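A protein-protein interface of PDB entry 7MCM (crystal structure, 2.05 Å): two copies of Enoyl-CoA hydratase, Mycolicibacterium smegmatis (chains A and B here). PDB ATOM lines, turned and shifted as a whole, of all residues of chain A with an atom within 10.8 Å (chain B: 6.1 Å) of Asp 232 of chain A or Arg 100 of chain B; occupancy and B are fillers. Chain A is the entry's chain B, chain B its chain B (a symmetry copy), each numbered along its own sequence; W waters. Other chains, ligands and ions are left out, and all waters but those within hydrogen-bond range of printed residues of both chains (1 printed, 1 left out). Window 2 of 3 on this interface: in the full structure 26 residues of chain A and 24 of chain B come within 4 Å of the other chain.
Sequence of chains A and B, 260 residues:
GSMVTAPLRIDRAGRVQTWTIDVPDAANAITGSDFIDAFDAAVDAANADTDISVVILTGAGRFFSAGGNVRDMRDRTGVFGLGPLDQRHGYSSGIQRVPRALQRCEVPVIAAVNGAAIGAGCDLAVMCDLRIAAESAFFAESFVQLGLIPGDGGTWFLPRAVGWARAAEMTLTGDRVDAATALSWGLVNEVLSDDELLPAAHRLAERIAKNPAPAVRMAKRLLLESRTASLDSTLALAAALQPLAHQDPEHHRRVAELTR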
ATOM      1  N   LEU A 222     -17.910  -9.976  10.171  1.00  0.00           N
ATOM      2  CA  LEU A 222     -18.017 -10.277   8.749  1.00  0.00           C
ATOM      3  C   LEU A 222     -18.708  -9.151   7.996  1.00  0.00           C
ATOM      4  O   LEU A 222     -18.270  -8.771   6.905  1.00  0.00           O
ATOM      5  CB  LEU A 222     -18.781 -11.582   8.559  1.00  0.00           C
ATOM      6  CG  LEU A 222     -17.935 -12.788   8.221  1.00  0.00           C
ATOM      7  CD1 LEU A 222     -18.843 -13.958   7.837  1.00  0.00           C
ATOM      8  CD2 LEU A 222     -16.941 -12.473   7.127  1.00  0.00           C
ATOM      9  N   GLU A 225     -16.306  -6.330   7.462  1.00  0.00           N
ATOM     10  CA  GLU A 225     -15.341  -6.629   6.407  1.00  0.00           C
ATOM     11  C   GLU A 225     -15.932  -6.414   5.018  1.00  0.00           C
ATOM     12  O   GLU A 225     -15.233  -5.952   4.107  1.00  0.00           O
ATOM     13  CB  GLU A 225     -14.839  -8.068   6.578  1.00  0.00           C
ATOM     14  CG  GLU A 225     -13.952  -8.556   5.452  1.00  0.00           C
ATOM     15  CD  GLU A 225     -12.508  -8.160   5.668  1.00  0.00           C
ATOM     16  OE1 GLU A 225     -12.219  -7.509   6.695  1.00  0.00           O
ATOM     17  OE2 GLU A 225     -11.668  -8.465   4.795  1.00  0.00           O
ATOM     18  N   SER A 226     -17.224  -6.695   4.846  1.00  0.00           N
ATOM     19  CA  SER A 226     -17.823  -6.631   3.520  1.00  0.00           C
ATOM     20  C   SER A 226     -17.991  -5.200   3.006  1.00  0.00           C
ATOM     21  O   SER A 226     -18.091  -5.004   1.786  1.00  0.00           O
ATOM     22  CB  SER A 226     -19.159  -7.371   3.554  1.00  0.00           C
ATOM     23  OG  SER A 226     -18.991  -8.674   4.127  1.00  0.00           O
ATOM     24  N   THR A 228     -15.873  -2.924   2.671  1.00  0.00           N
ATOM     25  CA  THR A 228     -14.744  -2.456   1.873  1.00  0.00           C
ATOM     26  C   THR A 228     -14.005  -3.569   1.145  1.00  0.00           C
ATOM     27  O   THR A 228     -13.557  -3.364   0.013  1.00  0.00           O
ATOM     28  CB  THR A 228     -13.752  -1.708   2.773  1.00  0.00           C
ATOM     29  OG1 THR A 228     -13.664  -2.385   4.034  1.00  0.00           O
ATOM     30  CG2 THR A 228     -14.187  -0.259   2.979  1.00  0.00           C
ATOM     31  N   ALA A 229     -13.859  -4.731   1.763  1.00  0.00           N
ATOM     32  CA  ALA A 229     -12.980  -5.755   1.229  1.00  0.00           C
ATOM     33  C   ALA A 229     -13.551  -6.377  -0.044  1.00  0.00           C
ATOM     34  O   ALA A 229     -14.744  -6.284  -0.344  1.00  0.00           O
ATOM     35  CB  ALA A 229     -12.740  -6.840   2.277  1.00  0.00           C
ATOM     36  N   SER A 230     -12.666  -7.014  -0.803  1.00  0.00           N
ATOM     37  CA  SER A 230     -13.067  -7.762  -1.983  1.00  0.00           C
ATOM     38  C   SER A 230     -13.939  -8.952  -1.584  1.00  0.00           C
ATOM     39  O   SER A 230     -14.035  -9.326  -0.409  1.00  0.00           O
ATOM     40  CB  SER A 230     -11.835  -8.279  -2.719  1.00  0.00           C
ATOM     41  OG  SER A 230     -11.192  -9.256  -1.897  1.00  0.00           O
ATOM     42  N   LEU A 231     -14.571  -9.572  -2.582  1.00  0.00           N
ATOM     43  CA  LEU A 231     -15.266 -10.820  -2.296  1.00  0.00           C
ATOM     44  C   LEU A 231     -14.298 -11.865  -1.757  1.00  0.00           C
ATOM     45  O   LEU A 231     -14.607 -12.566  -0.788  1.00  0.00           O
ATOM     46  CB  LEU A 231     -15.980 -11.329  -3.546  1.00  0.00           C
ATOM     47  CG  LEU A 231     -16.616 -12.718  -3.431  1.00  0.00           C
ATOM     48  CD1 LEU A 231     -17.611 -12.802  -2.268  1.00  0.00           C
ATOM     49  CD2 LEU A 231     -17.304 -13.048  -4.738  1.00  0.00           C
ATOM     50  N   ASP A 232     -13.108 -11.956  -2.351  1.00  0.00           N
ATOM     51  CA  ASP A 232     -12.132 -12.958  -1.934  1.00  0.00           C
ATOM     52  C   ASP A 232     -11.748 -12.795  -0.465  1.00  0.00           C
ATOM     53  O   ASP A 232     -11.545 -13.788   0.245  1.00  0.00           O
ATOM     54  CB  ASP A 232     -10.889 -12.879  -2.824  1.00  0.00           C
ATOM     55  CG  ASP A 232     -11.131 -13.441  -4.213  1.00  0.00           C
ATOM     56  OD1 ASP A 232     -11.988 -14.342  -4.347  1.00  0.00           O
ATOM     57  OD2 ASP A 232     -10.463 -12.987  -5.167  1.00  0.00           O
ATOM     58  N   SER A 233     -11.612 -11.555  -0.003  1.00  0.00           N
ATOM     59  CA  SER A 233     -11.277 -11.319   1.395  1.00  0.00           C
ATOM     60  C   SER A 233     -12.392 -11.788   2.318  1.00  0.00           C
ATOM     61  O   SER A 233     -12.125 -12.352   3.386  1.00  0.00           O
ATOM     62  CB  SER A 233     -10.986  -9.840   1.621  1.00  0.00           C
ATOM     63  OG  SER A 233      -9.763  -9.504   1.004  1.00  0.00           O
ATOM     64  N   THR A 234     -13.648 -11.533   1.938  1.00  0.00           N
ATOM     65  CA  THR A 234     -14.768 -11.968   2.762  1.00  0.00           C
ATOM     66  C   THR A 234     -14.852 -13.489   2.800  1.00  0.00           C
ATOM     67  O   THR A 234     -15.105 -14.077   3.859  1.00  0.00           O
ATOM     68  CB  THR A 234     -16.068 -11.359   2.240  1.00  0.00           C
ATOM     69  OG1 THR A 234     -16.021  -9.936   2.389  1.00  0.00           O
ATOM     70  CG2 THR A 234     -17.291 -11.928   2.977  1.00  0.00           C
ATOM     71  N   LEU A 235     -14.617 -14.140   1.656  1.00  0.00           N
ATOM     72  CA  LEU A 235     -14.638 -15.597   1.618  1.00  0.00           C
ATOM     73  C   LEU A 235     -13.555 -16.186   2.514  1.00  0.00           C
ATOM     74  O   LEU A 235     -13.795 -17.168   3.224  1.00  0.00           O
ATOM     75  CB  LEU A 235     -14.472 -16.086   0.176  1.00  0.00           C
ATOM     76  CG  LEU A 235     -15.628 -15.814  -0.797  1.00  0.00           C
ATOM     77  CD1 LEU A 235     -15.240 -16.231  -2.221  1.00  0.00           C
ATOM     78  CD2 LEU A 235     -16.887 -16.528  -0.349  1.00  0.00           C
ATOM     79  N   ALA A 236     -12.353 -15.601   2.494  1.00  0.00           N
ATOM     80  CA  ALA A 236     -11.268 -16.090   3.339  1.00  0.00           C
ATOM     81  C   ALA A 236     -11.587 -15.910   4.822  1.00  0.00           C
ATOM     82  O   ALA A 236     -11.306 -16.799   5.635  1.00  0.00           O
ATOM     83  CB  ALA A 236      -9.966 -15.365   2.983  1.00  0.00           C
ATOM     84  N   LEU A 237     -12.145 -14.755   5.196  1.00  0.00           N
ATOM     85  CA  LEU A 237     -12.472 -14.508   6.598  1.00  0.00           C
ATOM     86  C   LEU A 237     -13.609 -15.414   7.052  1.00  0.00           C
ATOM     87  O   LEU A 237     -13.534 -16.027   8.120  1.00  0.00           O
ATOM     88  CB  LEU A 237     -12.829 -13.037   6.811  1.00  0.00           C
ATOM     89  CG  LEU A 237     -13.130 -12.569   8.249  1.00  0.00           C
ATOM     90  CD1 LEU A 237     -11.937 -12.811   9.186  1.00  0.00           C
ATOM     91  CD2 LEU A 237     -13.550 -11.104   8.287  1.00  0.00           C
ATOM     92  N   ALA A 238     -14.666 -15.517   6.245  1.00  0.00           N
ATOM     93  CA  ALA A 238     -15.778 -16.387   6.609  1.00  0.00           C
ATOM     94  C   ALA A 238     -15.305 -17.822   6.823  1.00  0.00           C
ATOM     95  O   ALA A 238     -15.713 -18.478   7.788  1.00  0.00           O
ATOM     96  CB  ALA A 238     -16.864 -16.334   5.536  1.00  0.00           C
ATOM     97  N   ALA A 239     -14.424 -18.319   5.947  1.00  0.00           N
ATOM     98  CA  ALA A 239     -13.884 -19.667   6.113  1.00  0.00           C
ATOM     99  C   ALA A 239     -13.077 -19.786   7.395  1.00  0.00           C
ATOM    100  O   ALA A 239     -13.131 -20.816   8.082  1.00  0.00           O
ATOM    101  CB  ALA A 239     -13.026 -20.039   4.905  1.00  0.00           C
ATOM    102  N   ALA A 240     -12.315 -18.745   7.731  1.00  0.00           N
ATOM    103  CA  ALA A 240     -11.499 -18.778   8.937  1.00  0.00           C
ATOM    104  C   ALA A 240     -12.339 -18.644  10.204  1.00  0.00           C
ATOM    105  O   ALA A 240     -11.963 -19.178  11.251  1.00  0.00           O
ATOM    106  CB  ALA A 240     -10.444 -17.675   8.886  1.00  0.00           C
ATOM    107  N   ASP B  40     -21.009 -26.189 -11.011  1.00  0.00           N
ATOM    108  CA  ASP B  40     -19.773 -25.920 -11.738  1.00  0.00           C
ATOM    109  C   ASP B  40     -19.921 -26.253 -13.219  1.00  0.00           C
ATOM    110  O   ASP B  40     -19.618 -25.427 -14.084  1.00  0.00           O
ATOM    111  CB  ASP B  40     -18.615 -26.724 -11.143  1.00  0.00           C
ATOM    112  CG  ASP B  40     -17.846 -25.956 -10.088  1.00  0.00           C
ATOM    113  OD1 ASP B  40     -17.834 -24.706 -10.123  1.00  0.00           O
ATOM    114  OD2 ASP B  40     -17.246 -26.612  -9.213  1.00  0.00           O
ATOM    115  N   SER B  93     -12.788 -23.664  -0.071  1.00  0.00           N
ATOM    116  CA  SER B  93     -13.760 -24.367   0.762  1.00  0.00           C
ATOM    117  C   SER B  93     -14.953 -24.813  -0.103  1.00  0.00           C
ATOM    118  O   SER B  93     -15.271 -24.170  -1.102  1.00  0.00           O
ATOM    119  CB  SER B  93     -14.207 -23.481   1.933  1.00  0.00           C
ATOM    120  OG  SER B  93     -15.082 -24.172   2.808  1.00  0.00           O
ATOM    121  N   GLN B  96     -17.977 -22.719  -0.911  1.00  0.00           N
ATOM    122  CA  GLN B  96     -17.580 -21.500  -1.599  1.00  0.00           C
ATOM    123  C   GLN B  96     -17.371 -21.700  -3.093  1.00  0.00           C
ATOM    124  O   GLN B  96     -17.167 -20.716  -3.809  1.00  0.00           O
ATOM    125  CB  GLN B  96     -16.317 -20.930  -0.949  1.00  0.00           C
ATOM    126  CG  GLN B  96     -16.573 -20.391   0.457  1.00  0.00           C
ATOM    127  CD  GLN B  96     -15.365 -19.708   1.077  1.00  0.00           C
ATOM    128  OE1 GLN B  96     -14.266 -19.724   0.520  1.00  0.00           O
ATOM    129  NE2 GLN B  96     -15.569 -19.104   2.251  1.00  0.00           N
ATOM    130  N   ARG B  97     -17.476 -22.940  -3.582  1.00  0.00           N
ATOM    131  CA  ARG B  97     -17.377 -23.189  -5.016  1.00  0.00           C
ATOM    132  C   ARG B  97     -18.548 -22.567  -5.769  1.00  0.00           C
ATOM    133  O   ARG B  97     -18.379 -22.089  -6.894  1.00  0.00           O
ATOM    134  CB  ARG B  97     -17.295 -24.692  -5.276  1.00  0.00           C
ATOM    135  CG  ARG B  97     -15.950 -25.298  -4.929  1.00  0.00           C
ATOM    136  CD  ARG B  97     -15.968 -26.813  -5.071  1.00  0.00           C
ATOM    137  NE  ARG B  97     -16.321 -27.241  -6.418  1.00  0.00           N
ATOM    138  CZ  ARG B  97     -16.610 -28.495  -6.742  1.00  0.00           C
ATOM    139  NH1 ARG B  97     -16.594 -29.461  -5.836  1.00  0.00           N
ATOM    140  NH2 ARG B  97     -16.910 -28.788  -8.005  1.00  0.00           N
ATOM    141  N   VAL B  98     -19.752 -22.602  -5.186  1.00  0.00           N
ATOM    142  CA  VAL B  98     -20.918 -22.005  -5.849  1.00  0.00           C
ATOM    143  C   VAL B  98     -20.766 -20.499  -6.047  1.00  0.00           C
ATOM    144  O   VAL B  98     -20.975 -20.022  -7.177  1.00  0.00           O
ATOM    145  CB  VAL B  98     -22.204 -22.372  -5.083  1.00  0.00           C
ATOM    146  CG1 VAL B  98     -23.341 -21.415  -5.449  1.00  0.00           C
ATOM    147  CG2 VAL B  98     -22.590 -23.795  -5.366  1.00  0.00           C
ATOM    148  N   PRO B  99     -20.410 -19.699  -5.028  1.00  0.00           N
ATOM    149  CA  PRO B  99     -20.170 -18.270  -5.288  1.00  0.00           C
ATOM    150  C   PRO B  99     -19.109 -18.034  -6.343  1.00  0.00           C
ATOM    151  O   PRO B  99     -19.269 -17.157  -7.201  1.00  0.00           O
ATOM    152  CB  PRO B  99     -19.715 -17.735  -3.925  1.00  0.00           C
ATOM    153  CG  PRO B  99     -20.183 -18.715  -2.950  1.00  0.00           C
ATOM    154  CD  PRO B  99     -20.243 -20.028  -3.601  1.00  0.00           C
ATOM    155  N   ARG B 100     -18.028 -18.813  -6.309  1.00  0.00           N
ATOM    156  CA  ARG B 100     -16.964 -18.621  -7.281  1.00  0.00           C
ATOM    157  C   ARG B 100     -17.430 -19.003  -8.677  1.00  0.00           C
ATOM    158  O   ARG B 100     -16.996 -18.392  -9.660  1.00  0.00           O
ATOM    159  CB  ARG B 100     -15.734 -19.439  -6.882  1.00  0.00           C
ATOM    160  CG  ARG B 100     -15.100 -18.974  -5.573  1.00  0.00           C
ATOM    161  CD  ARG B 100     -13.731 -19.581  -5.358  1.00  0.00           C
ATOM    162  NE  ARG B 100     -13.186 -19.208  -4.058  1.00  0.00           N
ATOM    163  CZ  ARG B 100     -12.596 -18.048  -3.799  1.00  0.00           C
ATOM    164  NH1 ARG B 100     -12.463 -17.116  -4.730  1.00  0.00           N
ATOM    165  NH2 ARG B 100     -12.152 -17.808  -2.565  1.00  0.00           N
ATOM    166  N   ALA B 101     -18.314 -19.999  -8.786  1.00  0.00           N
ATOM    167  CA  ALA B 101     -18.862 -20.352 -10.095  1.00  0.00           C
ATOM    168  C   ALA B 101     -19.687 -19.202 -10.670  1.00  0.00           C
ATOM    169  O   ALA B 101     -19.540 -18.837 -11.844  1.00  0.00           O
ATOM    170  CB  ALA B 101     -19.693 -21.631  -9.990  1.00  0.00           C
ATOM    171  N   LEU B 102     -20.546 -18.596  -9.843  1.00  0.00           N
ATOM    172  CA  LEU B 102     -21.353 -17.482 -10.326  1.00  0.00           C
ATOM    173  C   LEU B 102     -20.476 -16.301 -10.700  1.00  0.00           C
ATOM    174  O   LEU B 102     -20.814 -15.540 -11.613  1.00  0.00           O
ATOM    175  CB  LEU B 102     -22.375 -17.091  -9.261  1.00  0.00           C
ATOM    176  CG  LEU B 102     -23.710 -17.808  -9.411  1.00  0.00           C
ATOM    177  CD1 LEU B 102     -24.642 -17.355  -8.321  1.00  0.00           C
ATOM    178  CD2 LEU B 102     -24.305 -17.555 -10.801  1.00  0.00           C
ATOM    179  N   GLN B 103     -19.331 -16.157 -10.025  1.00  0.00           N
ATOM    180  CA  GLN B 103     -18.392 -15.090 -10.344  1.00  0.00           C
ATOM    181  C   GLN B 103     -17.783 -15.261 -11.718  1.00  0.00           C
ATOM    182  O   GLN B 103     -17.415 -14.269 -12.347  1.00  0.00           O
ATOM    183  CB  GLN B 103     -17.264 -15.042  -9.311  1.00  0.00           C
ATOM    184  CG  GLN B 103     -17.570 -14.300  -8.024  1.00  0.00           C
ATOM    185  CD  GLN B 103     -17.916 -12.839  -8.272  1.00  0.00           C
ATOM    186  OE1 GLN B 103     -19.075 -12.425  -8.166  1.00  0.00           O
ATOM    187  NE2 GLN B 103     -16.895 -12.044  -8.601  1.00  0.00           N
ATOM    188  N   ARG B 104     -17.610 -16.495 -12.176  1.00  0.00           N
ATOM    189  CA  ARG B 104     -17.069 -16.708 -13.507  1.00  0.00           C
ATOM    190  C   ARG B 104     -18.157 -16.954 -14.547  1.00  0.00           C
ATOM    191  O   ARG B 104     -17.839 -17.118 -15.731  1.00  0.00           O
ATOM    192  CB  ARG B 104     -16.047 -17.851 -13.494  1.00  0.00           C
ATOM    193  CG  ARG B 104     -16.646 -19.225 -13.402  1.00  0.00           C
ATOM    194  CD  ARG B 104     -15.605 -20.340 -13.585  1.00  0.00           C
ATOM    195  NE  ARG B 104     -16.245 -21.650 -13.501  1.00  0.00           N
ATOM    196  CZ  ARG B 104     -16.447 -22.304 -12.363  1.00  0.00           C
ATOM    197  NH1 ARG B 104     -16.022 -21.823 -11.203  1.00  0.00           N
ATOM    198  NH2 ARG B 104     -17.093 -23.469 -12.387  1.00  0.00           N
ATOM    199  N   CYS B 105     -19.431 -16.942 -14.143  1.00  0.00           N
ATOM    200  CA  CYS B 105     -20.526 -17.098 -15.096  1.00  0.00           C
ATOM    201  C   CYS B 105     -20.690 -15.835 -15.927  1.00  0.00           C
ATOM    202  O   CYS B 105     -21.012 -14.768 -15.387  1.00  0.00           O
ATOM    203  CB  CYS B 105     -21.829 -17.417 -14.373  1.00  0.00           C
ATOM    204  SG  CYS B 105     -23.189 -17.824 -15.506  1.00  0.00           S
ATOM    205  N   TRP B 156     -21.153 -10.529   1.875  1.00  0.00           N
ATOM    206  CA  TRP B 156     -20.678  -9.580   0.868  1.00  0.00           C
ATOM    207  C   TRP B 156     -21.801  -9.168  -0.082  1.00  0.00           C
ATOM    208  O   TRP B 156     -21.947  -7.981  -0.402  1.00  0.00           O
ATOM    209  CB  TRP B 156     -19.497 -10.182   0.106  1.00  0.00           C
ATOM    210  CG  TRP B 156     -18.720  -9.214  -0.758  1.00  0.00           C
ATOM    211  CD1 TRP B 156     -17.658  -8.441  -0.387  1.00  0.00           C
ATOM    212  CD2 TRP B 156     -18.930  -8.961  -2.153  1.00  0.00           C
ATOM    213  NE1 TRP B 156     -17.206  -7.707  -1.457  1.00  0.00           N
ATOM    214  CE2 TRP B 156     -17.971  -8.006  -2.556  1.00  0.00           C
ATOM    215  CE3 TRP B 156     -19.842  -9.435  -3.093  1.00  0.00           C
ATOM    216  CZ2 TRP B 156     -17.890  -7.529  -3.873  1.00  0.00           C
ATOM    217  CZ3 TRP B 156     -19.764  -8.957  -4.406  1.00  0.00           C
ATOM    218  CH2 TRP B 156     -18.799  -8.012  -4.777  1.00  0.00           C
HETATM  219  O   HOH W   1     -10.855 -16.314  -0.570  1.00  0.00           O
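N of Leu 231 of chain A sits close to NE1 of Trp 156 of chain B (3.4 Å). The backbone carbonyl oxygen (O) of Leu 235 of chain A sits at hydrogen-bond distance from the side-chain amide nitrogen (NE2) of Gln 96 of chain B (2.8 Å). The backbone carbonyl oxygen of Ala 229 of chain A is in hydrogen-bond range of the indole nitrogen of Trp 156 of chain B, 3.1 Å away. The side-chain carboxylate of Asp 232 of chain A is in salt-bridge range of the guanidinium group of Arg 100 of chain B, 2.8 Å away.
O of Leu 222 of chain A sits at hydrogen-bond distance from OG of Ser 226 of chain A (2.9 Å). N of Ser 233 of chain A lies within hydrogen-bond range of OG of Ser 230 of chain A (3.0 Å). OG of Ser 230 of chain A sits close to N of Asp 232 of chain A, 3.3 Å away. O of Ser 230 of chain A sits at hydrogen-bond distance from OG1 of Thr 234 of chain A (3.5 Å).
Trp 156 of chain B touches Ser 226 of chain A (N to OG, 3.6 Å). Ser 230 of chain A touches Trp 156 of chain B (C to NE1, 3.5 Å). CD2 of Leu 231 of chain A touches CG of Gln 103 of chain B, 3.5 Å away. Thr 234 of chain A touches Trp 156 of chain B. Arg 100 of chain B touches Leu 235 of chain A. NE2 of Gln 96 of chain B touches CB of Ala 239 of chain A, at 3.8 Å.
Of the printed residues of chain B, Ala 229 of chain A touches Trp 156 (3.1 Å). Printed residues of chain B within 4 Å of Leu 231 of chain A: Gln 103 (3.5 Å) and Trp 156 (3.4 Å). Asp 232 of chain A touches just one residue of chain B: Arg 100. Of the printed residues of chain B, Thr 234 of chain A touches Trp 156 (3.6 Å). Of the printed residues of chain B, Leu 235 of chain A touches Gln 96 (2.8 Å) and Arg 100 (3.5 Å). Of chain A, only Leu 235 (2.8 Å) and Ala 239 (3.8 Å) come within 4 Å of Gln 96 of chain B. No residue of chain A comes within 4 Å of Pro 99 of chain B. Of chain A, only Asp 232 and Leu 235 come within 4 Å of Arg 100 of chain B. No residue of chain A comes within 4 Å of Arg 104 of chain B. The nearest residue of chain B that does not touch Asp 232 of chain A is Trp 156 of chain B (6.0 Å). The nearest residue of chain A that does not touch Arg 100 of chain B is Ala 236 of chain A (5.5 Å). The nearest printed residue of chain B that does not touch Ala 229 of chain A is Gln 103 of chain B (10.3 Å).
Of the 13 printed residues of chain B, 4 touch a printed residue of chain A. Of the 16 printed residues of chain A, 8 touch a printed residue of chain B. Hydrophobic or aromatic side chains of chain A within 4 Å of the printed part of chain B: Leu 231, Leu 235 and Ala 239. Among the printed residues, 10 pairs touch across the chains. Among the printed residues, Asp or Glu carboxylates within 4 Å of a Lys or Arg side-chain nitrogen of the other chain: Asp 232 of chain A with Arg 100 of chain B.
No position is printed for both chains.
Water W1 lies within hydrogen-bond range of the backbone carbonyl oxygen of Asp 232 of chain A, the guanidinium group of Arg 100 of chain B and the backbone NH of Ala 236 of chain A.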
